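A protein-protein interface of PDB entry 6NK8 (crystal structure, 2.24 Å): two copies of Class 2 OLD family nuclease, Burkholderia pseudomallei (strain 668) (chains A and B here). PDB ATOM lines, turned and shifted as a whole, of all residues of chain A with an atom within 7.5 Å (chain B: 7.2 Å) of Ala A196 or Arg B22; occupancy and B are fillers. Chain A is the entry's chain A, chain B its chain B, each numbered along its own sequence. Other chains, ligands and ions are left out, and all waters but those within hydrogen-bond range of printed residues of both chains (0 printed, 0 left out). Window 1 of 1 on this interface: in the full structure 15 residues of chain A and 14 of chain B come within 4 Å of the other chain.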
ATOM      1  N   PHE A  34      12.104 -20.114  28.966  1.00  0.00           N
ATOM      2  CA  PHE A  34      12.580 -18.747  29.095  1.00  0.00           C
ATOM      3  C   PHE A  34      12.321 -18.151  30.473  1.00  0.00           C
ATOM      4  O   PHE A  34      13.105 -17.305  30.921  1.00  0.00           O
ATOM      5  CB  PHE A  34      11.934 -17.871  28.026  1.00  0.00           C
ATOM      6  CG  PHE A  34      12.450 -18.148  26.642  1.00  0.00           C
ATOM      7  CD1 PHE A  34      13.680 -17.650  26.234  1.00  0.00           C
ATOM      8  CD2 PHE A  34      11.722 -18.914  25.760  1.00  0.00           C
ATOM      9  CE1 PHE A  34      14.160 -17.909  24.959  1.00  0.00           C
ATOM     10  CE2 PHE A  34      12.198 -19.191  24.500  1.00  0.00           C
ATOM     11  CZ  PHE A  34      13.420 -18.680  24.094  1.00  0.00           C
ATOM     12  N   LEU A  35      11.263 -18.581  31.173  1.00  0.00           N
ATOM     13  CA  LEU A  35      10.920 -17.902  32.412  1.00  0.00           C
ATOM     14  C   LEU A  35      11.613 -18.479  33.629  1.00  0.00           C
ATOM     15  O   LEU A  35      11.912 -17.732  34.563  1.00  0.00           O
ATOM     16  CB  LEU A  35       9.408 -17.922  32.652  1.00  0.00           C
ATOM     17  CG  LEU A  35       8.628 -16.959  31.749  1.00  0.00           C
ATOM     18  CD1 LEU A  35       7.161 -17.326  31.783  1.00  0.00           C
ATOM     19  CD2 LEU A  35       8.854 -15.522  32.187  1.00  0.00           C
ATOM     20  N   GLY A 147       2.887  -6.768  33.663  1.00  0.00           N
ATOM     21  CA  GLY A 147       3.857  -7.110  32.645  1.00  0.00           C
ATOM     22  C   GLY A 147       3.224  -7.837  31.482  1.00  0.00           C
ATOM     23  O   GLY A 147       3.510  -7.530  30.324  1.00  0.00           O
ATOM     24  N   VAL A 151       3.423  -6.498  27.724  1.00  0.00           N
ATOM     25  CA  VAL A 151       3.985  -7.302  26.647  1.00  0.00           C
ATOM     26  C   VAL A 151       2.972  -7.446  25.520  1.00  0.00           C
ATOM     27  O   VAL A 151       3.287  -7.243  24.340  1.00  0.00           O
ATOM     28  CB  VAL A 151       4.443  -8.672  27.187  1.00  0.00           C
ATOM     29  CG1 VAL A 151       4.766  -9.614  26.040  1.00  0.00           C
ATOM     30  CG2 VAL A 151       5.658  -8.515  28.101  1.00  0.00           C
ATOM     31  N   ILE A 152       1.736  -7.782  25.869  1.00  0.00           N
ATOM     32  CA  ILE A 152       0.726  -8.057  24.854  1.00  0.00           C
ATOM     33  C   ILE A 152       0.391  -6.787  24.094  1.00  0.00           C
ATOM     34  O   ILE A 152       0.326  -6.785  22.859  1.00  0.00           O
ATOM     35  CB  ILE A 152      -0.529  -8.674  25.499  1.00  0.00           C
ATOM     36  CG1 ILE A 152      -0.204 -10.077  26.030  1.00  0.00           C
ATOM     37  CG2 ILE A 152      -1.680  -8.694  24.511  1.00  0.00           C
ATOM     38  CD1 ILE A 152      -1.364 -10.810  26.653  1.00  0.00           C
ATOM     39  N   SER A 154       2.208  -4.142  23.667  1.00  0.00           N
ATOM     40  CA  SER A 154       3.279  -3.559  22.869  1.00  0.00           C
ATOM     41  C   SER A 154       3.716  -4.444  21.715  1.00  0.00           C
ATOM     42  O   SER A 154       4.341  -3.949  20.775  1.00  0.00           O
ATOM     43  CB  SER A 154       4.483  -3.215  23.744  1.00  0.00           C
ATOM     44  OG  SER A 154       4.634  -4.144  24.780  1.00  0.00           O
ATOM     45  N   GLU A 155       3.390  -5.726  21.736  1.00  0.00           N
ATOM     46  CA  GLU A 155       3.815  -6.601  20.657  1.00  0.00           C
ATOM     47  C   GLU A 155       2.733  -6.818  19.620  1.00  0.00           C
ATOM     48  O   GLU A 155       3.042  -6.986  18.439  1.00  0.00           O
ATOM     49  CB  GLU A 155       4.269  -7.963  21.218  1.00  0.00           C
ATOM     50  CG  GLU A 155       5.547  -7.855  22.062  1.00  0.00           C
ATOM     51  CD  GLU A 155       6.597  -8.938  21.777  1.00  0.00           C
ATOM     52  OE1 GLU A 155       7.669  -8.886  22.410  1.00  0.00           O
ATOM     53  OE2 GLU A 155       6.357  -9.842  20.940  1.00  0.00           O
ATOM     54  N   ILE A 188       1.725 -14.091  19.497  1.00  0.00           N
ATOM     55  CA  ILE A 188       3.115 -13.719  19.690  1.00  0.00           C
ATOM     56  C   ILE A 188       4.007 -14.931  19.513  1.00  0.00           C
ATOM     57  O   ILE A 188       5.115 -14.836  18.983  1.00  0.00           O
ATOM     58  CB  ILE A 188       3.289 -13.092  21.089  1.00  0.00           C
ATOM     59  CG1 ILE A 188       2.433 -11.838  21.222  1.00  0.00           C
ATOM     60  CG2 ILE A 188       4.771 -12.801  21.373  1.00  0.00           C
ATOM     61  CD1 ILE A 188       2.305 -11.322  22.628  1.00  0.00           C
ATOM     62  N   LYS A 190       4.536 -18.539  22.152  1.00  0.00           N
ATOM     63  CA  LYS A 190       4.687 -18.734  23.588  1.00  0.00           C
ATOM     64  C   LYS A 190       6.113 -18.460  24.039  1.00  0.00           C
ATOM     65  O   LYS A 190       6.333 -17.895  25.119  1.00  0.00           O
ATOM     66  CB  LYS A 190       4.247 -20.147  23.960  1.00  0.00           C
ATOM     67  CG  LYS A 190       2.977 -20.164  24.806  1.00  0.00           C
ATOM     68  CD  LYS A 190       2.077 -21.380  24.539  1.00  0.00           C
ATOM     69  CE  LYS A 190       1.043 -21.497  25.663  1.00  0.00           C
ATOM     70  NZ  LYS A 190       0.407 -22.828  25.783  1.00  0.00           N
ATOM     71  N   GLY A 191       7.094 -18.823  23.214  1.00  0.00           N
ATOM     72  CA  GLY A 191       8.478 -18.565  23.578  1.00  0.00           C
ATOM     73  C   GLY A 191       8.866 -17.104  23.431  1.00  0.00           C
ATOM     74  O   GLY A 191       9.583 -16.558  24.271  1.00  0.00           O
ATOM     75  N   ARG A 192       8.428 -16.458  22.348  1.00  0.00           N
ATOM     76  CA  ARG A 192       8.642 -15.021  22.209  1.00  0.00           C
ATOM     77  C   ARG A 192       7.958 -14.261  23.341  1.00  0.00           C
ATOM     78  O   ARG A 192       8.555 -13.388  23.973  1.00  0.00           O
ATOM     79  CB  ARG A 192       8.122 -14.545  20.851  1.00  0.00           C
ATOM     80  CG  ARG A 192       8.968 -15.006  19.677  1.00  0.00           C
ATOM     81  CD  ARG A 192       8.406 -14.512  18.324  1.00  0.00           C
ATOM     82  NE  ARG A 192       9.040 -15.161  17.178  1.00  0.00           N
ATOM     83  CZ  ARG A 192      10.296 -14.943  16.794  1.00  0.00           C
ATOM     84  NH1 ARG A 192      11.054 -14.095  17.474  1.00  0.00           N
ATOM     85  NH2 ARG A 192      10.799 -15.579  15.737  1.00  0.00           N
ATOM     86  N   PHE A 193       6.706 -14.599  23.622  1.00  0.00           N
ATOM     87  CA  PHE A 193       5.999 -13.977  24.730  1.00  0.00           C
ATOM     88  C   PHE A 193       6.792 -14.100  26.027  1.00  0.00           C
ATOM     89  O   PHE A 193       7.030 -13.109  26.718  1.00  0.00           O
ATOM     90  CB  PHE A 193       4.610 -14.607  24.883  1.00  0.00           C
ATOM     91  CG  PHE A 193       3.884 -14.149  26.112  1.00  0.00           C
ATOM     92  CD1 PHE A 193       3.301 -12.892  26.159  1.00  0.00           C
ATOM     93  CD2 PHE A 193       3.777 -14.970  27.218  1.00  0.00           C
ATOM     94  CE1 PHE A 193       2.635 -12.465  27.305  1.00  0.00           C
ATOM     95  CE2 PHE A 193       3.118 -14.553  28.343  1.00  0.00           C
ATOM     96  CZ  PHE A 193       2.547 -13.297  28.388  1.00  0.00           C
ATOM     97  N   ALA A 194       7.217 -15.314  26.362  1.00  0.00           N
ATOM     98  CA  ALA A 194       7.902 -15.549  27.626  1.00  0.00           C
ATOM     99  C   ALA A 194       9.239 -14.841  27.683  1.00  0.00           C
ATOM    100  O   ALA A 194       9.657 -14.383  28.754  1.00  0.00           O
ATOM    101  CB  ALA A 194       8.102 -17.044  27.844  1.00  0.00           C
ATOM    102  N   GLN A 195       9.947 -14.762  26.555  1.00  0.00           N
ATOM    103  CA  GLN A 195      11.215 -14.044  26.577  1.00  0.00           C
ATOM    104  C   GLN A 195      10.989 -12.564  26.859  1.00  0.00           C
ATOM    105  O   GLN A 195      11.747 -11.947  27.612  1.00  0.00           O
ATOM    106  CB  GLN A 195      11.993 -14.217  25.265  1.00  0.00           C
ATOM    107  CG  GLN A 195      13.345 -13.506  25.354  1.00  0.00           C
ATOM    108  CD  GLN A 195      14.180 -13.560  24.089  1.00  0.00           C
ATOM    109  OE1 GLN A 195      13.794 -13.019  23.042  1.00  0.00           O
ATOM    110  NE2 GLN A 195      15.346 -14.196  24.182  1.00  0.00           N
ATOM    111  N   ALA A 196       9.963 -11.968  26.249  1.00  0.00           N
ATOM    112  CA  ALA A 196       9.648 -10.581  26.580  1.00  0.00           C
ATOM    113  C   ALA A 196       9.244 -10.458  28.045  1.00  0.00           C
ATOM    114  O   ALA A 196       9.663  -9.530  28.741  1.00  0.00           O
ATOM    115  CB  ALA A 196       8.538 -10.061  25.661  1.00  0.00           C
ATOM    116  N   LEU A 197       8.465 -11.411  28.543  1.00  0.00           N
ATOM    117  CA  LEU A 197       7.980 -11.297  29.910  1.00  0.00           C
ATOM    118  C   LEU A 197       9.104 -11.489  30.921  1.00  0.00           C
ATOM    119  O   LEU A 197       9.032 -10.962  32.033  1.00  0.00           O
ATOM    120  CB  LEU A 197       6.871 -12.319  30.144  1.00  0.00           C
ATOM    121  CG  LEU A 197       6.227 -12.267  31.528  1.00  0.00           C
ATOM    122  CD1 LEU A 197       5.476 -10.943  31.691  1.00  0.00           C
ATOM    123  CD2 LEU A 197       5.296 -13.461  31.717  1.00  0.00           C
ATOM    124  N   ALA A 198      10.138 -12.251  30.559  1.00  0.00           N
ATOM    125  CA  ALA A 198      11.285 -12.442  31.442  1.00  0.00           C
ATOM    126  C   ALA A 198      11.844 -11.128  31.951  1.00  0.00           C
ATOM    127  O   ALA A 198      12.355 -11.080  33.073  1.00  0.00           O
ATOM    128  CB  ALA A 198      12.387 -13.205  30.707  1.00  0.00           C
ATOM    129  N   GLY A 199      11.772 -10.056  31.143  1.00  0.00           N
ATOM    130  CA  GLY A 199      12.317  -8.767  31.544  1.00  0.00           C
ATOM    131  C   GLY A 199      11.622  -8.163  32.754  1.00  0.00           C
ATOM    132  O   GLY A 199      12.170  -7.247  33.385  1.00  0.00           O
ATOM    133  N   PHE A 200      10.430  -8.662  33.095  1.00  0.00           N
ATOM    134  CA  PHE A 200       9.688  -8.219  34.273  1.00  0.00           C
ATOM    135  C   PHE A 200       9.851  -9.149  35.454  1.00  0.00           C
ATOM    136  O   PHE A 200       9.234  -8.914  36.482  1.00  0.00           O
ATOM    137  CB  PHE A 200       8.192  -8.096  33.961  1.00  0.00           C
ATOM    138  CG  PHE A 200       7.881  -7.057  32.954  1.00  0.00           C
ATOM    139  CD1 PHE A 200       7.931  -7.347  31.617  1.00  0.00           C
ATOM    140  CD2 PHE A 200       7.576  -5.770  33.349  1.00  0.00           C
ATOM    141  CE1 PHE A 200       7.664  -6.368  30.675  1.00  0.00           C
ATOM    142  CE2 PHE A 200       7.308  -4.785  32.410  1.00  0.00           C
ATOM    143  CZ  PHE A 200       7.359  -5.089  31.076  1.00  0.00           C
ATOM    144  N   ALA A 201      10.636 -10.208  35.323  1.00  0.00           N
ATOM    145  CA  ALA A 201      10.767 -11.172  36.401  1.00  0.00           C
ATOM    146  C   ALA A 201      11.339 -10.517  37.656  1.00  0.00           C
ATOM    147  O   ALA A 201      12.322  -9.772  37.591  1.00  0.00           O
ATOM    148  CB  ALA A 201      11.658 -12.321  35.941  1.00  0.00           C
ATOM    149  N   PHE B  19      17.472 -18.348  17.531  1.00  0.00           N
ATOM    150  CA  PHE B  19      17.849 -17.078  18.159  1.00  0.00           C
ATOM    151  C   PHE B  19      16.665 -16.096  18.332  1.00  0.00           C
ATOM    152  O   PHE B  19      15.606 -16.470  18.842  1.00  0.00           O
ATOM    153  CB  PHE B  19      18.987 -16.382  17.379  1.00  0.00           C
ATOM    154  CG  PHE B  19      18.626 -15.969  15.958  1.00  0.00           C
ATOM    155  CD1 PHE B  19      18.701 -14.637  15.597  1.00  0.00           C
ATOM    156  CD2 PHE B  19      18.300 -16.923  14.974  1.00  0.00           C
ATOM    157  CE1 PHE B  19      18.400 -14.240  14.290  1.00  0.00           C
ATOM    158  CE2 PHE B  19      17.989 -16.572  13.648  1.00  0.00           C
ATOM    159  CZ  PHE B  19      18.048 -15.224  13.296  1.00  0.00           C
ATOM    160  N   PHE B  20      16.881 -14.844  17.900  1.00  0.00           N
ATOM    161  CA  PHE B  20      16.020 -13.675  18.118  1.00  0.00           C
ATOM    162  C   PHE B  20      16.056 -13.260  19.588  1.00  0.00           C
ATOM    163  O   PHE B  20      15.073 -12.761  20.148  1.00  0.00           O
ATOM    164  CB  PHE B  20      14.589 -13.921  17.629  1.00  0.00           C
ATOM    165  CG  PHE B  20      14.389 -13.625  16.168  1.00  0.00           C
ATOM    166  CD1 PHE B  20      15.480 -13.703  15.317  1.00  0.00           C
ATOM    167  CD2 PHE B  20      13.107 -13.303  15.647  1.00  0.00           C
ATOM    168  CE1 PHE B  20      15.335 -13.445  13.947  1.00  0.00           C
ATOM    169  CE2 PHE B  20      12.897 -13.042  14.313  1.00  0.00           C
ATOM    170  CZ  PHE B  20      14.036 -13.115  13.418  1.00  0.00           C
ATOM    171  N   ALA B  21      17.225 -13.453  20.197  1.00  0.00           N
ATOM    172  CA  ALA B  21      17.553 -12.871  21.482  1.00  0.00           C
ATOM    173  C   ALA B  21      17.505 -11.350  21.405  1.00  0.00           C
ATOM    174  O   ALA B  21      17.550 -10.756  20.320  1.00  0.00           O
ATOM    175  CB  ALA B  21      18.948 -13.328  21.898  1.00  0.00           C
ATOM    176  N   ARG B  22      17.416 -10.703  22.573  1.00  0.00           N
ATOM    177  CA  ARG B  22      17.584  -9.258  22.563  1.00  0.00           C
ATOM    178  C   ARG B  22      19.043  -8.865  22.441  1.00  0.00           C
ATOM    179  O   ARG B  22      19.327  -7.739  22.045  1.00  0.00           O
ATOM    180  CB  ARG B  22      16.972  -8.612  23.806  1.00  0.00           C
ATOM    181  CG  ARG B  22      15.678  -9.249  24.266  1.00  0.00           C
ATOM    182  CD  ARG B  22      14.519  -8.899  23.381  1.00  0.00           C
ATOM    183  NE  ARG B  22      13.649 -10.054  23.146  1.00  0.00           N
ATOM    184  CZ  ARG B  22      12.332 -10.058  23.351  1.00  0.00           C
ATOM    185  NH1 ARG B  22      11.720  -8.963  23.809  1.00  0.00           N
ATOM    186  NH2 ARG B  22      11.624 -11.157  23.102  1.00  0.00           N
ATOM    187  N   GLY B  23      19.973  -9.770  22.734  1.00  0.00           N
ATOM    188  CA  GLY B  23      21.390  -9.477  22.585  1.00  0.00           C
ATOM    189  C   GLY B  23      22.159 -10.774  22.484  1.00  0.00           C
ATOM    190  O   GLY B  23      21.666 -11.836  22.874  1.00  0.00           O
ATOM    191  N   ILE B  24      23.366 -10.693  21.927  1.00  0.00           N
ATOM    192  CA  ILE B  24      24.156 -11.890  21.678  1.00  0.00           C
ATOM    193  C   ILE B  24      25.583 -11.647  22.130  1.00  0.00           C
ATOM    194  O   ILE B  24      26.163 -10.596  21.845  1.00  0.00           O
ATOM    195  CB  ILE B  24      24.129 -12.329  20.201  1.00  0.00           C
ATOM    196  CG1 ILE B  24      22.709 -12.700  19.776  1.00  0.00           C
ATOM    197  CG2 ILE B  24      24.986 -13.573  20.016  1.00  0.00           C
ATOM    198  CD1 ILE B  24      22.499 -12.589  18.270  1.00  0.00           C
ATOM    199  N   ILE B  49      17.138 -12.409  32.229  1.00  0.00           N
ATOM    200  CA  ILE B  49      16.152 -11.335  32.327  1.00  0.00           C
ATOM    201  C   ILE B  49      16.254 -10.404  31.122  1.00  0.00           C
ATOM    202  O   ILE B  49      15.240  -9.955  30.581  1.00  0.00           O
ATOM    203  CB  ILE B  49      16.324 -10.589  33.661  1.00  0.00           C
ATOM    204  CG1 ILE B  49      15.867 -11.511  34.799  1.00  0.00           C
ATOM    205  CG2 ILE B  49      15.584  -9.218  33.656  1.00  0.00           C
ATOM    206  CD1 ILE B  49      16.108 -10.958  36.201  1.00  0.00           C
ATOM    207  N   LEU B  50      17.477 -10.109  30.675  1.00  0.00           N
ATOM    208  CA  LEU B  50      17.686  -9.200  29.555  1.00  0.00           C
ATOM    209  C   LEU B  50      17.540  -9.867  28.196  1.00  0.00           C
ATOM    210  O   LEU B  50      17.585  -9.164  27.180  1.00  0.00           O
ATOM    211  CB  LEU B  50      19.069  -8.566  29.667  1.00  0.00           C
ATOM    212  CG  LEU B  50      19.273  -7.688  30.925  1.00  0.00           C
ATOM    213  CD1 LEU B  50      20.689  -7.172  30.985  1.00  0.00           C
ATOM    214  CD2 LEU B  50      18.334  -6.510  30.892  1.00  0.00           C
ATOM    215  N   GLY B  51      17.363 -11.190  28.140  1.00  0.00           N
ATOM    216  CA  GLY B  51      17.224 -11.839  26.852  1.00  0.00           C
ATOM    217  C   GLY B  51      18.520 -11.934  26.081  1.00  0.00           C
ATOM    218  O   GLY B  51      18.504 -11.924  24.845  1.00  0.00           O
ATOM    219  N   ILE B  52      19.651 -12.047  26.776  1.00  0.00           N
ATOM    220  CA  ILE B  52      20.956 -12.092  26.133  1.00  0.00           C
ATOM    221  C   ILE B  52      21.408 -13.540  26.008  1.00  0.00           C
ATOM    222  O   ILE B  52      21.281 -14.326  26.949  1.00  0.00           O
ATOM    223  CB  ILE B  52      21.986 -11.258  26.901  1.00  0.00           C
ATOM    224  CG1 ILE B  52      21.610  -9.782  26.809  1.00  0.00           C
ATOM    225  CG2 ILE B  52      23.373 -11.509  26.323  1.00  0.00           C
ATOM    226  CD1 ILE B  52      22.208  -8.911  27.870  1.00  0.00           C
ATOM    227  N   SER B  53      21.912 -13.902  24.839  1.00  0.00           N
ATOM    228  CA  SER B  53      22.329 -15.262  24.575  1.00  0.00           C
ATOM    229  C   SER B  53      23.817 -15.284  24.287  1.00  0.00           C
ATOM    230  O   SER B  53      24.383 -14.309  23.788  1.00  0.00           O
ATOM    231  CB  SER B  53      21.563 -15.859  23.390  1.00  0.00           C
ATOM    232  OG  SER B  53      20.428 -16.563  23.851  1.00  0.00           O
ATOM    233  N   ASN B  75      20.278  -6.023  12.890  1.00  0.00           N
ATOM    234  CA  ASN B  75      20.600  -4.931  13.815  1.00  0.00           C
ATOM    235  C   ASN B  75      20.369  -5.323  15.276  1.00  0.00           C
ATOM    236  O   ASN B  75      19.631  -4.664  16.015  1.00  0.00           O
ATOM    237  CB  ASN B  75      19.802  -3.676  13.474  1.00  0.00           C
ATOM    238  CG  ASN B  75      20.444  -2.419  14.022  1.00  0.00           C
ATOM    239  OD1 ASN B  75      21.676  -2.298  14.055  1.00  0.00           O
ATOM    240  ND2 ASN B  75      19.615  -1.469  14.454  1.00  0.00           N
ATOM    241  N   ILE B  76      21.001  -6.405  15.698  1.00  0.00           N
ATOM    242  CA  ILE B  76      20.840  -6.936  17.049  1.00  0.00           C
ATOM    243  C   ILE B  76      22.069  -6.548  17.868  1.00  0.00           C
ATOM    244  O   ILE B  76      23.201  -6.720  17.381  1.00  0.00           O
ATOM    245  CB  ILE B  76      20.641  -8.463  17.038  1.00  0.00           C
ATOM    246  CG1 ILE B  76      19.391  -8.822  16.232  1.00  0.00           C
ATOM    247  CG2 ILE B  76      20.548  -9.025  18.463  1.00  0.00           C
ATOM    248  CD1 ILE B  76      19.119 -10.318  16.173  1.00  0.00           C
ATOM    249  N   PRO B  77      21.898  -6.001  19.071  1.00  0.00           N
ATOM    250  CA  PRO B  77      23.065  -5.711  19.920  1.00  0.00           C
ATOM    251  C   PRO B  77      23.877  -6.972  20.161  1.00  0.00           C
ATOM    252  O   PRO B  77      23.326  -8.045  20.410  1.00  0.00           O
ATOM    253  CB  PRO B  77      22.439  -5.184  21.209  1.00  0.00           C
ATOM    254  CG  PRO B  77      21.104  -4.640  20.765  1.00  0.00           C
ATOM    255  CD  PRO B  77      20.645  -5.478  19.637  1.00  0.00           C
ATOM    256  N   HIS B  78      25.197  -6.853  20.028  1.00  0.00           N
ATOM    257  CA  HIS B  78      26.042  -8.028  20.122  1.00  0.00           C
ATOM    258  C   HIS B  78      27.438  -7.620  20.576  1.00  0.00           C
ATOM    259  O   HIS B  78      27.843  -6.472  20.422  1.00  0.00           O
ATOM    260  CB  HIS B  78      26.103  -8.770  18.779  1.00  0.00           C
ATOM    261  CG  HIS B  78      26.671  -7.938  17.681  1.00  0.00           C
ATOM    262  ND1 HIS B  78      25.924  -6.993  17.007  1.00  0.00           N
ATOM    263  CD2 HIS B  78      27.926  -7.864  17.176  1.00  0.00           C
ATOM    264  CE1 HIS B  78      26.697  -6.377  16.128  1.00  0.00           C
ATOM    265  NE2 HIS B  78      27.912  -6.895  16.203  1.00  0.00           N
ATOM    266  N   ILE B 217      27.335  -5.430  26.665  1.00  0.00           N
ATOM    267  CA  ILE B 217      26.117  -5.988  26.078  1.00  0.00           C
ATOM    268  C   ILE B 217      24.919  -5.744  26.987  1.00  0.00           C
ATOM    269  O   ILE B 217      23.802  -5.519  26.495  1.00  0.00           O
ATOM    270  CB  ILE B 217      26.284  -7.486  25.723  1.00  0.00           C
ATOM    271  CG1 ILE B 217      25.093  -8.000  24.879  1.00  0.00           C
ATOM    272  CG2 ILE B 217      26.418  -8.365  26.955  1.00  0.00           C
ATOM    273  CD1 ILE B 217      24.893  -7.250  23.565  1.00  0.00           C
ATOM    274  N   ALA B 220      24.047  -2.191  26.046  1.00  0.00           N
ATOM    275  CA  ALA B 220      23.493  -2.079  24.699  1.00  0.00           C
ATOM    276  C   ALA B 220      22.033  -2.513  24.676  1.00  0.00           C
ATOM    277  O   ALA B 220      21.203  -1.883  24.018  1.00  0.00           O
ATOM    278  CB  ALA B 220      24.315  -2.900  23.705  1.00  0.00           C
ATOM    279  N   VAL B 221      21.699  -3.581  25.398  1.00  0.00           N
ATOM    280  CA  VAL B 221      20.333  -4.086  25.399  1.00  0.00           C
ATOM    281  C   VAL B 221      19.398  -3.163  26.179  1.00  0.00           C
ATOM    282  O   VAL B 221      18.232  -2.994  25.806  1.00  0.00           O
ATOM    283  CB  VAL B 221      20.314  -5.515  25.962  1.00  0.00           C
ATOM    284  CG1 VAL B 221      18.896  -6.041  26.060  1.00  0.00           C
ATOM    285  CG2 VAL B 221      21.188  -6.448  25.112  1.00  0.00           C
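No position is printed for both chains.
Arg A192 touches Phe B20 (NH1 to CD2, 2.9 Å). Arg B22 touches Arg A192. Gln A195 touches Ala B21 (NE2 to CA, 3.7 Å). Gln A195 touches Gly B51 (NE2 to O, 3.9 Å). N of Ala A196 touches NH2 of Arg B22 (3.6 Å). Ile B49 touches Ala A198. Gly A199 touches Ile B49.
Glu A155 touches none of the printed residues of chain B. Of the printed residues of chain B, Gln A195 touches Phe B20, Ala B21, Arg B22 and Gly B51. Ala A196 touches one residue of chain B. Printed residues of chain B within 4 Å of Ala A198: Ile B49 (3.8 Å). Printed residues of chain A within 4 Å of Ala B21: Gln A195 (3.7 Å). Arg B22 touches just these residues of chain A: Arg A192, Gln A195 and Ala A196. Ile B24 touches none of the printed residues of chain A. The nearest residue of chain A that does not touch Arg B22 is Glu A155 (4.3 Å).
Of the 20 printed residues of chain A, 5 touch a printed residue of chain B. Of the 18 printed residues of chain B, 5 touch a printed residue of chain A. Printed residues of chain B that touch a printed residue of chain A: Phe B20, Ala B21, Arg B22, Ile B49 and Gly B51. Hydrophobic or aromatic side chains of chain B within 4 Å of the printed part of chain A: Phe B20 and Ile B49. Among the printed residues, no Asp or Glu carboxylate lies within 4 Å of a Lys or Arg side-chain nitrogen of the other chain.
The backbone NH of Arg B22 sits at hydrogen-bond distance from the backbone carbonyl oxygen of Gly B51 (2.8 Å). O of Gly B51 lies within hydrogen-bond range of N of Gly B23, at 3.4 Å.
O of Phe B20 lies close to OE1 of Gln A195, at 3.2 Å. OE1 of Gln A195 lies within hydrogen-bond range of NH2 of Arg B22 (2.9 Å).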
